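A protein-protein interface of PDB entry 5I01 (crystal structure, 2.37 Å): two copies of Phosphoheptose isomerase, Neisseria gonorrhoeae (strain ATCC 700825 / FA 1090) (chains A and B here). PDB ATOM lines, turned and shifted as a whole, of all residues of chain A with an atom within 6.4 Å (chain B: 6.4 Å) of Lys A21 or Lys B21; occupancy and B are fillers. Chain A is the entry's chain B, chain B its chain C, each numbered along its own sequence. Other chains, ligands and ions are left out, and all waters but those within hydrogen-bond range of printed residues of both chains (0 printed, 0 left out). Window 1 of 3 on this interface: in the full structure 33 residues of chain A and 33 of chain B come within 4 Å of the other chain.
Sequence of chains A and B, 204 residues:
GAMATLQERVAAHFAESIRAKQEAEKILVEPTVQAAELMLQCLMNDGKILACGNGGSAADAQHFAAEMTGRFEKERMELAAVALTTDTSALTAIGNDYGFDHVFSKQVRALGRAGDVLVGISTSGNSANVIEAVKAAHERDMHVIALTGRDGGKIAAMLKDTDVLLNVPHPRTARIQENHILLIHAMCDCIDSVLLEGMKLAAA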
ATOM      1  N   PHE A  14      17.683  13.319 -12.549  1.00  0.00           N
ATOM      2  CA  PHE A  14      17.669  14.577 -11.786  1.00  0.00           C
ATOM      3  C   PHE A  14      16.490  14.641 -10.807  1.00  0.00           C
ATOM      4  O   PHE A  14      16.669  14.916  -9.614  1.00  0.00           O
ATOM      5  CB  PHE A  14      17.604  15.784 -12.732  1.00  0.00           C
ATOM      6  CG  PHE A  14      18.946  16.292 -13.194  1.00  0.00           C
ATOM      7  CD1 PHE A  14      19.679  17.184 -12.403  1.00  0.00           C
ATOM      8  CD2 PHE A  14      19.460  15.928 -14.441  1.00  0.00           C
ATOM      9  CE1 PHE A  14      20.907  17.689 -12.844  1.00  0.00           C
ATOM     10  CE2 PHE A  14      20.686  16.422 -14.885  1.00  0.00           C
ATOM     11  CZ  PHE A  14      21.406  17.307 -14.088  1.00  0.00           C
ATOM     12  N   GLU A  16      14.509  12.140  -9.716  1.00  0.00           N
ATOM     13  CA  GLU A  16      14.693  11.086  -8.714  1.00  0.00           C
ATOM     14  C   GLU A  16      15.676  11.528  -7.612  1.00  0.00           C
ATOM     15  O   GLU A  16      15.403  11.348  -6.423  1.00  0.00           O
ATOM     16  CB  GLU A  16      15.138   9.770  -9.369  1.00  0.00           C
ATOM     17  CG  GLU A  16      14.967   8.527  -8.499  1.00  0.00           C
ATOM     18  CD  GLU A  16      15.316   7.235  -9.230  1.00  0.00           C
ATOM     19  OE1 GLU A  16      16.491   7.068  -9.611  1.00  0.00           O
ATOM     20  OE2 GLU A  16      14.422   6.377  -9.417  1.00  0.00           O
ATOM     21  N   SER A  17      16.788  12.147  -8.016  1.00  0.00           N
ATOM     22  CA  SER A  17      17.821  12.628  -7.083  1.00  0.00           C
ATOM     23  C   SER A  17      17.366  13.793  -6.205  1.00  0.00           C
ATOM     24  O   SER A  17      17.768  13.877  -5.043  1.00  0.00           O
ATOM     25  CB  SER A  17      19.081  13.040  -7.841  1.00  0.00           C
ATOM     26  OG  SER A  17      20.122  13.354  -6.931  1.00  0.00           O
ATOM     27  N   ILE A  18      16.557  14.695  -6.763  1.00  0.00           N
ATOM     28  CA  ILE A  18      15.916  15.740  -5.950  1.00  0.00           C
ATOM     29  C   ILE A  18      14.970  15.103  -4.915  1.00  0.00           C
ATOM     30  O   ILE A  18      15.038  15.442  -3.739  1.00  0.00           O
ATOM     31  CB  ILE A  18      15.165  16.788  -6.813  1.00  0.00           C
ATOM     32  CG1 ILE A  18      16.166  17.647  -7.594  1.00  0.00           C
ATOM     33  CG2 ILE A  18      14.289  17.688  -5.947  1.00  0.00           C
ATOM     34  CD1 ILE A  18      15.590  18.287  -8.843  1.00  0.00           C
ATOM     35  N   ARG A  19      14.104  14.184  -5.347  1.00  0.00           N
ATOM     36  CA  ARG A  19      13.177  13.517  -4.416  1.00  0.00           C
ATOM     37  C   ARG A  19      13.900  12.768  -3.314  1.00  0.00           C
ATOM     38  O   ARG A  19      13.472  12.813  -2.160  1.00  0.00           O
ATOM     39  CB  ARG A  19      12.277  12.506  -5.121  1.00  0.00           C
ATOM     40  CG  ARG A  19      11.116  13.104  -5.865  1.00  0.00           C
ATOM     41  CD  ARG A  19      10.038  12.062  -6.059  1.00  0.00           C
ATOM     42  NE  ARG A  19      10.532  10.782  -6.585  1.00  0.00           N
ATOM     43  CZ  ARG A  19      10.876  10.543  -7.854  1.00  0.00           C
ATOM     44  NH1 ARG A  19      10.834  11.506  -8.782  1.00  0.00           N
ATOM     45  NH2 ARG A  19      11.275   9.323  -8.201  1.00  0.00           N
ATOM     46  N   ALA A  20      14.966  12.057  -3.675  1.00  0.00           N
ATOM     47  CA  ALA A  20      15.733  11.284  -2.699  1.00  0.00           C
ATOM     48  C   ALA A  20      16.278  12.192  -1.632  1.00  0.00           C
ATOM     49  O   ALA A  20      16.228  11.844  -0.463  1.00  0.00           O
ATOM     50  CB  ALA A  20      16.859  10.519  -3.367  1.00  0.00           C
ATOM     51  N   LYS A  21      16.769  13.366  -2.043  1.00  0.00           N
ATOM     52  CA  LYS A  21      17.279  14.386  -1.110  1.00  0.00           C
ATOM     53  C   LYS A  21      16.209  15.084  -0.266  1.00  0.00           C
ATOM     54  O   LYS A  21      16.478  15.445   0.875  1.00  0.00           O
ATOM     55  CB  LYS A  21      18.127  15.427  -1.844  1.00  0.00           C
ATOM     56  CG  LYS A  21      19.542  14.949  -2.109  1.00  0.00           C
ATOM     57  CD  LYS A  21      20.275  15.855  -3.085  1.00  0.00           C
ATOM     58  CE  LYS A  21      21.766  15.544  -3.135  1.00  0.00           C
ATOM     59  NZ  LYS A  21      22.070  14.102  -3.352  1.00  0.00           N
ATOM     60  N   GLN A  22      15.016  15.286  -0.818  1.00  0.00           N
ATOM     61  CA  GLN A  22      13.895  15.827  -0.031  1.00  0.00           C
ATOM     62  C   GLN A  22      13.434  14.869   1.074  1.00  0.00           C
ATOM     63  O   GLN A  22      13.159  15.305   2.195  1.00  0.00           O
ATOM     64  CB  GLN A  22      12.728  16.225  -0.937  1.00  0.00           C
ATOM     65  CG  GLN A  22      12.997  17.535  -1.667  1.00  0.00           C
ATOM     66  CD  GLN A  22      12.048  17.812  -2.819  1.00  0.00           C
ATOM     67  OE1 GLN A  22      11.666  16.909  -3.560  1.00  0.00           O
ATOM     68  NE2 GLN A  22      11.681  19.076  -2.989  1.00  0.00           N
ATOM     69  N   GLU A  23      13.378  13.573   0.765  1.00  0.00           N
ATOM     70  CA  GLU A  23      13.006  12.550   1.750  1.00  0.00           C
ATOM     71  C   GLU A  23      14.113  12.323   2.762  1.00  0.00           C
ATOM     72  O   GLU A  23      13.851  12.220   3.957  1.00  0.00           O
ATOM     73  CB  GLU A  23      12.630  11.231   1.068  1.00  0.00           C
ATOM     74  CG  GLU A  23      11.426  11.315   0.126  1.00  0.00           C
ATOM     75  CD  GLU A  23      10.195  11.949   0.765  1.00  0.00           C
ATOM     76  OE1 GLU A  23       9.842  11.580   1.913  1.00  0.00           O
ATOM     77  OE2 GLU A  23       9.590  12.831   0.110  1.00  0.00           O
ATOM     78  N   ALA A  24      15.350  12.256   2.285  1.00  0.00           N
ATOM     79  CA  ALA A  24      16.518  12.161   3.170  1.00  0.00           C
ATOM     80  C   ALA A  24      16.597  13.314   4.186  1.00  0.00           C
ATOM     81  O   ALA A  24      16.916  13.079   5.350  1.00  0.00           O
ATOM     82  CB  ALA A  24      17.798  12.095   2.347  1.00  0.00           C
ATOM     83  N   GLU A  25      16.303  14.539   3.732  1.00  0.00           N
ATOM     84  CA  GLU A  25      16.267  15.748   4.585  1.00  0.00           C
ATOM     85  C   GLU A  25      15.370  15.596   5.823  1.00  0.00           C
ATOM     86  O   GLU A  25      15.720  16.076   6.892  1.00  0.00           O
ATOM     87  CB  GLU A  25      15.806  16.963   3.760  1.00  0.00           C
ATOM     88  CG  GLU A  25      15.871  18.313   4.474  1.00  0.00           C
ATOM     89  CD  GLU A  25      15.463  19.495   3.588  1.00  0.00           C
ATOM     90  OE1 GLU A  25      14.875  19.273   2.509  1.00  0.00           O
ATOM     91  OE2 GLU A  25      15.726  20.662   3.977  1.00  0.00           O
ATOM     92  N   LYS A  26      14.233  14.917   5.669  1.00  0.00           N
ATOM     93  CA  LYS A  26      13.273  14.724   6.763  1.00  0.00           C
ATOM     94  C   LYS A  26      13.739  13.801   7.901  1.00  0.00           C
ATOM     95  O   LYS A  26      13.232  13.935   9.012  1.00  0.00           O
ATOM     96  CB  LYS A  26      11.935  14.186   6.228  1.00  0.00           C
ATOM     97  CG  LYS A  26      11.188  15.118   5.289  1.00  0.00           C
ATOM     98  CD  LYS A  26       9.918  14.454   4.776  1.00  0.00           C
ATOM     99  CE  LYS A  26       9.244  15.259   3.677  1.00  0.00           C
ATOM    100  NZ  LYS A  26       7.830  14.827   3.476  1.00  0.00           N
ATOM    101  N   ARG A 175      21.456   6.786  -6.236  1.00  0.00           N
ATOM    102  CA  ARG A 175      20.863   7.806  -5.373  1.00  0.00           C
ATOM    103  C   ARG A 175      21.414   7.740  -3.945  1.00  0.00           C
ATOM    104  O   ARG A 175      21.499   8.769  -3.260  1.00  0.00           O
ATOM    105  CB  ARG A 175      19.345   7.636  -5.315  1.00  0.00           C
ATOM    106  CG  ARG A 175      18.642   7.665  -6.659  1.00  0.00           C
ATOM    107  CD  ARG A 175      18.689   9.031  -7.307  1.00  0.00           C
ATOM    108  NE  ARG A 175      19.824   9.186  -8.207  1.00  0.00           N
ATOM    109  CZ  ARG A 175      19.886   8.742  -9.466  1.00  0.00           C
ATOM    110  NH1 ARG A 175      20.981   8.974 -10.188  1.00  0.00           N
ATOM    111  NH2 ARG A 175      18.875   8.092 -10.033  1.00  0.00           N
ATOM    112  N   GLU A 178      24.896   9.347  -4.094  1.00  0.00           N
ATOM    113  CA  GLU A 178      24.705  10.800  -4.156  1.00  0.00           C
ATOM    114  C   GLU A 178      24.421  11.446  -2.793  1.00  0.00           C
ATOM    115  O   GLU A 178      24.972  12.508  -2.480  1.00  0.00           O
ATOM    116  CB  GLU A 178      23.621  11.159  -5.174  1.00  0.00           C
ATOM    117  CG  GLU A 178      24.107  11.040  -6.622  1.00  0.00           C
ATOM    118  CD  GLU A 178      23.010  10.676  -7.606  1.00  0.00           C
ATOM    119  OE1 GLU A 178      21.818  10.916  -7.292  1.00  0.00           O
ATOM    120  OE2 GLU A 178      23.340  10.117  -8.688  1.00  0.00           O
ATOM    121  N   ASN A 179      23.574  10.790  -2.000  1.00  0.00           N
ATOM    122  CA  ASN A 179      23.256  11.242  -0.640  1.00  0.00           C
ATOM    123  C   ASN A 179      24.417  11.032   0.342  1.00  0.00           C
ATOM    124  O   ASN A 179      24.580  11.817   1.277  1.00  0.00           O
ATOM    125  CB  ASN A 179      21.978  10.561  -0.107  1.00  0.00           C
ATOM    126  CG  ASN A 179      20.714  11.303  -0.503  1.00  0.00           C
ATOM    127  OD1 ASN A 179      20.169  12.053   0.295  1.00  0.00           O
ATOM    128  ND2 ASN A 179      20.253  11.118  -1.743  1.00  0.00           N
ATOM    129  N   HIS A 180      25.206   9.978   0.155  1.00  0.00           N
ATOM    130  CA  HIS A 180      26.365   9.755   1.008  1.00  0.00           C
ATOM    131  C   HIS A 180      27.384  10.892   0.905  1.00  0.00           C
ATOM    132  O   HIS A 180      27.928  11.332   1.923  1.00  0.00           O
ATOM    133  CB  HIS A 180      27.022   8.403   0.703  1.00  0.00           C
ATOM    134  CG  HIS A 180      26.297   7.234   1.288  1.00  0.00           C
ATOM    135  ND1 HIS A 180      26.659   5.931   1.024  1.00  0.00           N
ATOM    136  CD2 HIS A 180      25.231   7.166   2.120  1.00  0.00           C
ATOM    137  CE1 HIS A 180      25.852   5.110   1.674  1.00  0.00           C
ATOM    138  NE2 HIS A 180      24.982   5.835   2.351  1.00  0.00           N
ATOM    139  N   LEU A 182      26.733  14.020  -0.032  1.00  0.00           N
ATOM    140  CA  LEU A 182      26.106  15.144   0.670  1.00  0.00           C
ATOM    141  C   LEU A 182      26.290  15.047   2.192  1.00  0.00           C
ATOM    142  O   LEU A 182      26.609  16.044   2.830  1.00  0.00           O
ATOM    143  CB  LEU A 182      24.605  15.249   0.317  1.00  0.00           C
ATOM    144  CG  LEU A 182      23.749  16.264   1.093  1.00  0.00           C
ATOM    145  CD1 LEU A 182      24.317  17.663   0.985  1.00  0.00           C
ATOM    146  CD2 LEU A 182      22.318  16.257   0.590  1.00  0.00           C
ATOM    147  N   PHE B  14      21.319  20.507   3.030  1.00  0.00           N
ATOM    148  CA  PHE B  14      20.281  19.798   2.249  1.00  0.00           C
ATOM    149  C   PHE B  14      19.532  20.746   1.315  1.00  0.00           C
ATOM    150  O   PHE B  14      19.437  20.489   0.117  1.00  0.00           O
ATOM    151  CB  PHE B  14      19.274  19.074   3.161  1.00  0.00           C
ATOM    152  CG  PHE B  14      19.758  17.748   3.661  1.00  0.00           C
ATOM    153  CD1 PHE B  14      19.565  16.599   2.906  1.00  0.00           C
ATOM    154  CD2 PHE B  14      20.416  17.644   4.876  1.00  0.00           C
ATOM    155  CE1 PHE B  14      20.020  15.362   3.358  1.00  0.00           C
ATOM    156  CE2 PHE B  14      20.876  16.414   5.341  1.00  0.00           C
ATOM    157  CZ  PHE B  14      20.679  15.271   4.580  1.00  0.00           C
ATOM    158  N   GLU B  16      20.307  23.770   0.151  1.00  0.00           N
ATOM    159  CA  GLU B  16      21.170  24.279  -0.914  1.00  0.00           C
ATOM    160  C   GLU B  16      21.443  23.222  -2.006  1.00  0.00           C
ATOM    161  O   GLU B  16      21.433  23.550  -3.204  1.00  0.00           O
ATOM    162  CB  GLU B  16      22.484  24.830  -0.348  1.00  0.00           C
ATOM    163  CG  GLU B  16      23.260  25.690  -1.341  1.00  0.00           C
ATOM    164  CD  GLU B  16      24.595  26.179  -0.805  1.00  0.00           C
ATOM    165  OE1 GLU B  16      25.391  25.358  -0.296  1.00  0.00           O
ATOM    166  OE2 GLU B  16      24.862  27.390  -0.910  1.00  0.00           O
ATOM    167  N   SER B  17      21.669  21.967  -1.595  1.00  0.00           N
ATOM    168  CA  SER B  17      21.864  20.868  -2.541  1.00  0.00           C
ATOM    169  C   SER B  17      20.623  20.628  -3.406  1.00  0.00           C
ATOM    170  O   SER B  17      20.760  20.359  -4.609  1.00  0.00           O
ATOM    171  CB  SER B  17      22.263  19.579  -1.824  1.00  0.00           C
ATOM    172  OG  SER B  17      22.657  18.589  -2.763  1.00  0.00           O
ATOM    173  N   ILE B  18      19.429  20.747  -2.811  1.00  0.00           N
ATOM    174  CA  ILE B  18      18.172  20.720  -3.594  1.00  0.00           C
ATOM    175  C   ILE B  18      18.036  21.941  -4.531  1.00  0.00           C
ATOM    176  O   ILE B  18      17.678  21.765  -5.694  1.00  0.00           O
ATOM    177  CB  ILE B  18      16.918  20.566  -2.707  1.00  0.00           C
ATOM    178  CG1 ILE B  18      16.929  19.201  -2.022  1.00  0.00           C
ATOM    179  CG2 ILE B  18      15.634  20.706  -3.525  1.00  0.00           C
ATOM    180  CD1 ILE B  18      16.127  19.175  -0.736  1.00  0.00           C
ATOM    181  N   ARG B  19      18.324  23.154  -4.054  1.00  0.00           N
ATOM    182  CA  ARG B  19      18.300  24.330  -4.945  1.00  0.00           C
ATOM    183  C   ARG B  19      19.275  24.234  -6.124  1.00  0.00           C
ATOM    184  O   ARG B  19      18.940  24.682  -7.225  1.00  0.00           O
ATOM    185  CB  ARG B  19      18.566  25.638  -4.198  1.00  0.00           C
ATOM    186  CG  ARG B  19      17.372  26.184  -3.440  1.00  0.00           C
ATOM    187  CD  ARG B  19      17.593  27.630  -3.013  1.00  0.00           C
ATOM    188  NE  ARG B  19      18.921  27.879  -2.419  1.00  0.00           N
ATOM    189  CZ  ARG B  19      19.317  27.522  -1.185  1.00  0.00           C
ATOM    190  NH1 ARG B  19      18.509  26.862  -0.350  1.00  0.00           N
ATOM    191  NH2 ARG B  19      20.556  27.825  -0.780  1.00  0.00           N
ATOM    192  N   ALA B  20      20.468  23.670  -5.904  1.00  0.00           N
ATOM    193  CA  ALA B  20      21.476  23.560  -6.979  1.00  0.00           C
ATOM    194  C   ALA B  20      21.078  22.557  -8.054  1.00  0.00           C
ATOM    195  O   ALA B  20      21.258  22.810  -9.240  1.00  0.00           O
ATOM    196  CB  ALA B  20      22.841  23.209  -6.408  1.00  0.00           C
ATOM    197  N   LYS B  21      20.528  21.422  -7.637  1.00  0.00           N
ATOM    198  CA  LYS B  21      20.036  20.419  -8.583  1.00  0.00           C
ATOM    199  C   LYS B  21      18.827  20.925  -9.372  1.00  0.00           C
ATOM    200  O   LYS B  21      18.763  20.717 -10.570  1.00  0.00           O
ATOM    201  CB  LYS B  21      19.723  19.090  -7.883  1.00  0.00           C
ATOM    202  CG  LYS B  21      20.956  18.232  -7.627  1.00  0.00           C
ATOM    203  CD  LYS B  21      20.615  16.970  -6.849  1.00  0.00           C
ATOM    204  CE  LYS B  21      21.784  15.992  -6.785  1.00  0.00           C
ATOM    205  NZ  LYS B  21      23.054  16.591  -6.299  1.00  0.00           N
ATOM    206  N   GLN B  22      17.881  21.587  -8.710  1.00  0.00           N
ATOM    207  CA  GLN B  22      16.720  22.188  -9.402  1.00  0.00           C
ATOM    208  C   GLN B  22      17.171  23.201 -10.467  1.00  0.00           C
ATOM    209  O   GLN B  22      16.664  23.211 -11.583  1.00  0.00           O
ATOM    210  CB  GLN B  22      15.786  22.868  -8.400  1.00  0.00           C
ATOM    211  CG  GLN B  22      15.005  21.890  -7.537  1.00  0.00           C
ATOM    212  CD  GLN B  22      14.377  22.514  -6.289  1.00  0.00           C
ATOM    213  OE1 GLN B  22      14.895  23.476  -5.709  1.00  0.00           O
ATOM    214  NE2 GLN B  22      13.262  21.951  -5.861  1.00  0.00           N
ATOM    215  N   GLU B  23      18.145  24.029 -10.101  1.00  0.00           N
ATOM    216  CA  GLU B  23      18.773  24.991 -11.012  1.00  0.00           C
ATOM    217  C   GLU B  23      19.536  24.311 -12.158  1.00  0.00           C
ATOM    218  O   GLU B  23      19.504  24.786 -13.291  1.00  0.00           O
ATOM    219  CB  GLU B  23      19.719  25.905 -10.215  1.00  0.00           C
ATOM    220  CG  GLU B  23      20.353  27.047 -11.011  1.00  0.00           C
ATOM    221  CD  GLU B  23      21.264  27.933 -10.170  1.00  0.00           C
ATOM    222  OE1 GLU B  23      21.447  27.673  -8.956  1.00  0.00           O
ATOM    223  OE2 GLU B  23      21.804  28.903 -10.732  1.00  0.00           O
ATOM    224  N   ALA B  24      20.228  23.217 -11.841  1.00  0.00           N
ATOM    225  CA  ALA B  24      21.016  22.454 -12.811  1.00  0.00           C
ATOM    226  C   ALA B  24      20.175  21.634 -13.789  1.00  0.00           C
ATOM    227  O   ALA B  24      20.525  21.537 -14.961  1.00  0.00           O
ATOM    228  CB  ALA B  24      21.982  21.541 -12.078  1.00  0.00           C
ATOM    229  N   GLU B  25      19.096  21.030 -13.296  1.00  0.00           N
ATOM    230  CA  GLU B  25      18.197  20.176 -14.107  1.00  0.00           C
ATOM    231  C   GLU B  25      17.671  20.847 -15.392  1.00  0.00           C
ATOM    232  O   GLU B  25      17.512  20.180 -16.411  1.00  0.00           O
ATOM    233  CB  GLU B  25      17.012  19.688 -13.241  1.00  0.00           C
ATOM    234  CG  GLU B  25      15.820  19.090 -13.998  1.00  0.00           C
ATOM    235  CD  GLU B  25      14.761  18.480 -13.081  1.00  0.00           C
ATOM    236  OE1 GLU B  25      14.504  19.060 -11.997  1.00  0.00           O
ATOM    237  OE2 GLU B  25      14.183  17.423 -13.460  1.00  0.00           O
ATOM    238  N   LYS B  26      17.398  22.151 -15.332  1.00  0.00           N
ATOM    239  CA  LYS B  26      16.781  22.881 -16.453  1.00  0.00           C
ATOM    240  C   LYS B  26      17.731  23.196 -17.598  1.00  0.00           C
ATOM    241  O   LYS B  26      17.272  23.476 -18.703  1.00  0.00           O
ATOM    242  CB  LYS B  26      16.107  24.186 -15.978  1.00  0.00           C
ATOM    243  CG  LYS B  26      14.654  24.023 -15.541  1.00  0.00           C
ATOM    244  CD  LYS B  26      14.534  23.380 -14.174  1.00  0.00           C
ATOM    245  CE  LYS B  26      13.085  23.087 -13.821  1.00  0.00           C
ATOM    246  NZ  LYS B  26      12.934  22.980 -12.343  1.00  0.00           N
ATOM    247  N   ARG B 175      28.701  21.645  -3.779  1.00  0.00           N
ATOM    248  CA  ARG B 175      27.482  21.539  -4.582  1.00  0.00           C
ATOM    249  C   ARG B 175      27.788  21.143  -6.021  1.00  0.00           C
ATOM    250  O   ARG B 175      26.996  20.445  -6.650  1.00  0.00           O
ATOM    251  CB  ARG B 175      26.746  22.881  -4.581  1.00  0.00           C
ATOM    252  CG  ARG B 175      26.271  23.334  -3.205  1.00  0.00           C
ATOM    253  CD  ARG B 175      25.192  22.417  -2.649  1.00  0.00           C
ATOM    254  NE  ARG B 175      25.728  21.330  -1.830  1.00  0.00           N
ATOM    255  CZ  ARG B 175      26.158  21.452  -0.569  1.00  0.00           C
ATOM    256  NH1 ARG B 175      26.615  20.376   0.060  1.00  0.00           N
ATOM    257  NH2 ARG B 175      26.145  22.622   0.070  1.00  0.00           N
ATOM    258  N   GLU B 178      28.644  17.289  -6.077  1.00  0.00           N
ATOM    259  CA  GLU B 178      27.400  16.522  -5.984  1.00  0.00           C
ATOM    260  C   GLU B 178      26.675  16.422  -7.317  1.00  0.00           C
ATOM    261  O   GLU B 178      26.168  15.357  -7.670  1.00  0.00           O
ATOM    262  CB  GLU B 178      26.469  17.134  -4.940  1.00  0.00           C
ATOM    263  CG  GLU B 178      26.981  16.993  -3.506  1.00  0.00           C
ATOM    264  CD  GLU B 178      26.520  18.107  -2.579  1.00  0.00           C
ATOM    265  OE1 GLU B 178      25.575  18.845  -2.923  1.00  0.00           O
ATOM    266  OE2 GLU B 178      27.118  18.250  -1.488  1.00  0.00           O
ATOM    267  N   ASN B 179      26.618  17.526  -8.055  1.00  0.00           N
ATOM    268  CA  ASN B 179      26.022  17.489  -9.387  1.00  0.00           C
ATOM    269  C   ASN B 179      26.856  16.654 -10.367  1.00  0.00           C
ATOM    270  O   ASN B 179      26.286  15.973 -11.222  1.00  0.00           O
ATOM    271  CB  ASN B 179      25.729  18.905  -9.929  1.00  0.00           C
ATOM    272  CG  ASN B 179      24.383  19.449  -9.439  1.00  0.00           C
ATOM    273  OD1 ASN B 179      23.369  19.327 -10.128  1.00  0.00           O
ATOM    274  ND2 ASN B 179      24.362  20.007  -8.221  1.00  0.00           N
ATOM    275  N   ILE B 181      28.761  13.866  -9.801  1.00  0.00           N
ATOM    276  CA  ILE B 181      28.457  12.435  -9.608  1.00  0.00           C
ATOM    277  C   ILE B 181      27.105  12.061 -10.169  1.00  0.00           C
ATOM    278  O   ILE B 181      26.980  10.985 -10.737  1.00  0.00           O
ATOM    279  CB  ILE B 181      28.535  11.930  -8.143  1.00  0.00           C
ATOM    280  CG1 ILE B 181      27.652  12.789  -7.241  1.00  0.00           C
ATOM    281  CG2 ILE B 181      29.977  11.913  -7.656  1.00  0.00           C
ATOM    282  CD1 ILE B 181      27.660  12.425  -5.789  1.00  0.00           C
ATOM    283  N   LEU B 182      26.110  12.943 -10.032  1.00  0.00           N
ATOM    284  CA  LEU B 182      24.794  12.726 -10.653  1.00  0.00           C
ATOM    285  C   LEU B 182      24.871  12.723 -12.194  1.00  0.00           C
ATOM    286  O   LEU B 182      24.250  11.877 -12.850  1.00  0.00           O
ATOM    287  CB  LEU B 182      23.766  13.765 -10.181  1.00  0.00           C
ATOM    288  CG  LEU B 182      22.390  13.782 -10.882  1.00  0.00           C
ATOM    289  CD1 LEU B 182      21.670  12.453 -10.738  1.00  0.00           C
ATOM    290  CD2 LEU B 182      21.515  14.888 -10.331  1.00  0.00           C
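The side-chain carboxylate (OE1) of Glu A16 is in salt-bridge range of the guanidinium group (NH2) of Arg A175, at 2.6 Å. The side-chain carboxylate (OE1) of Glu A178 sits at hydrogen-bond distance from the side-chain hydroxyl (OG) of Ser A17, 3.0 Å away. The side-chain amino group of Lys A21 lies within hydrogen-bond range of the backbone carbonyl oxygen of Glu A178 (3.4 Å). The side-chain hydroxyl (OG) of Ser B17 is in hydrogen-bond range of the side-chain carboxylate (OE1) of Glu B178 (2.9 Å). O of Ile B18 sits close to OE1 of Gln B22 (3.3 Å). O of Arg B175 sits at hydrogen-bond distance from ND2 of Asn B179 (3.1 Å).
CA of Glu B25 touches CD1 of Phe A14 (3.7 Å). Phe A14 touches Leu B182 (CD1 to CD2, 3.6 Å). Ser A17 touches Lys B21. Ile A18 touches Lys B21. Ser B17 touches Lys A21 (OG to CE, 3.2 Å). Lys B21 touches Lys A21 (NZ to CE, 3.6 Å). Glu A25 touches Phe B14. Arg A175 touches Leu B182 (NH1 to CD1, 3.6 Å). OE2 of Glu A178 touches CD1 of Leu B182 (3.5 Å). NH1 of Arg B175 touches CD1 of Leu A182, at 3.7 Å.
Of the printed residues of chain B, Lys A21 touches Phe B14, Ser B17, Ile B18 and Lys B21. Lys B21 touches three residues of chain A. Printed residues of chain A within 4 Å of Ile B181: Glu A178 (3.7 Å). Printed residues of chain A within 4 Å of Leu B182: Phe A14 (3.6 Å), Ser A17 (3.9 Å), Arg A175 (3.6 Å) and Glu A178 (3.5 Å). The nearest residue of chain A that does not touch Lys B21 is Phe A14 (4.1 Å). The nearest printed residue of chain A that does not touch Phe B14 is Ala A24 (4.1 Å).
Along chain B the printed residues that touch a printed residue of chain A span positions 14 to 182. Among the printed residues, 21 pairs touch across the chains. Among the printed residues, no Asp or Glu carboxylate lies within 4 Å of a Lys or Arg side-chain nitrogen of the other chain.
Phe A14 touches Leu B182, and with the chains exchanged Leu A182 touches Phe B14. Ser A17 touches Lys B21, and with the chains exchanged Lys A21 touches Ser B17. Ile A18 touches Gln B22, and with the chains exchanged Gln A22 touches Ile B18. Glu A178 touches Leu B182, and with the chains exchanged Leu A182 touches Glu B178. Positions printed for both chains: 14, 16, 17, 18, 19, 20, 21, 22, 23, 24, 25, 26, 175, 178, 179 and 182. Of the 21 pairs that touch across the chains among the printed residues, 19 have their exchanged pair printed and touching as well.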
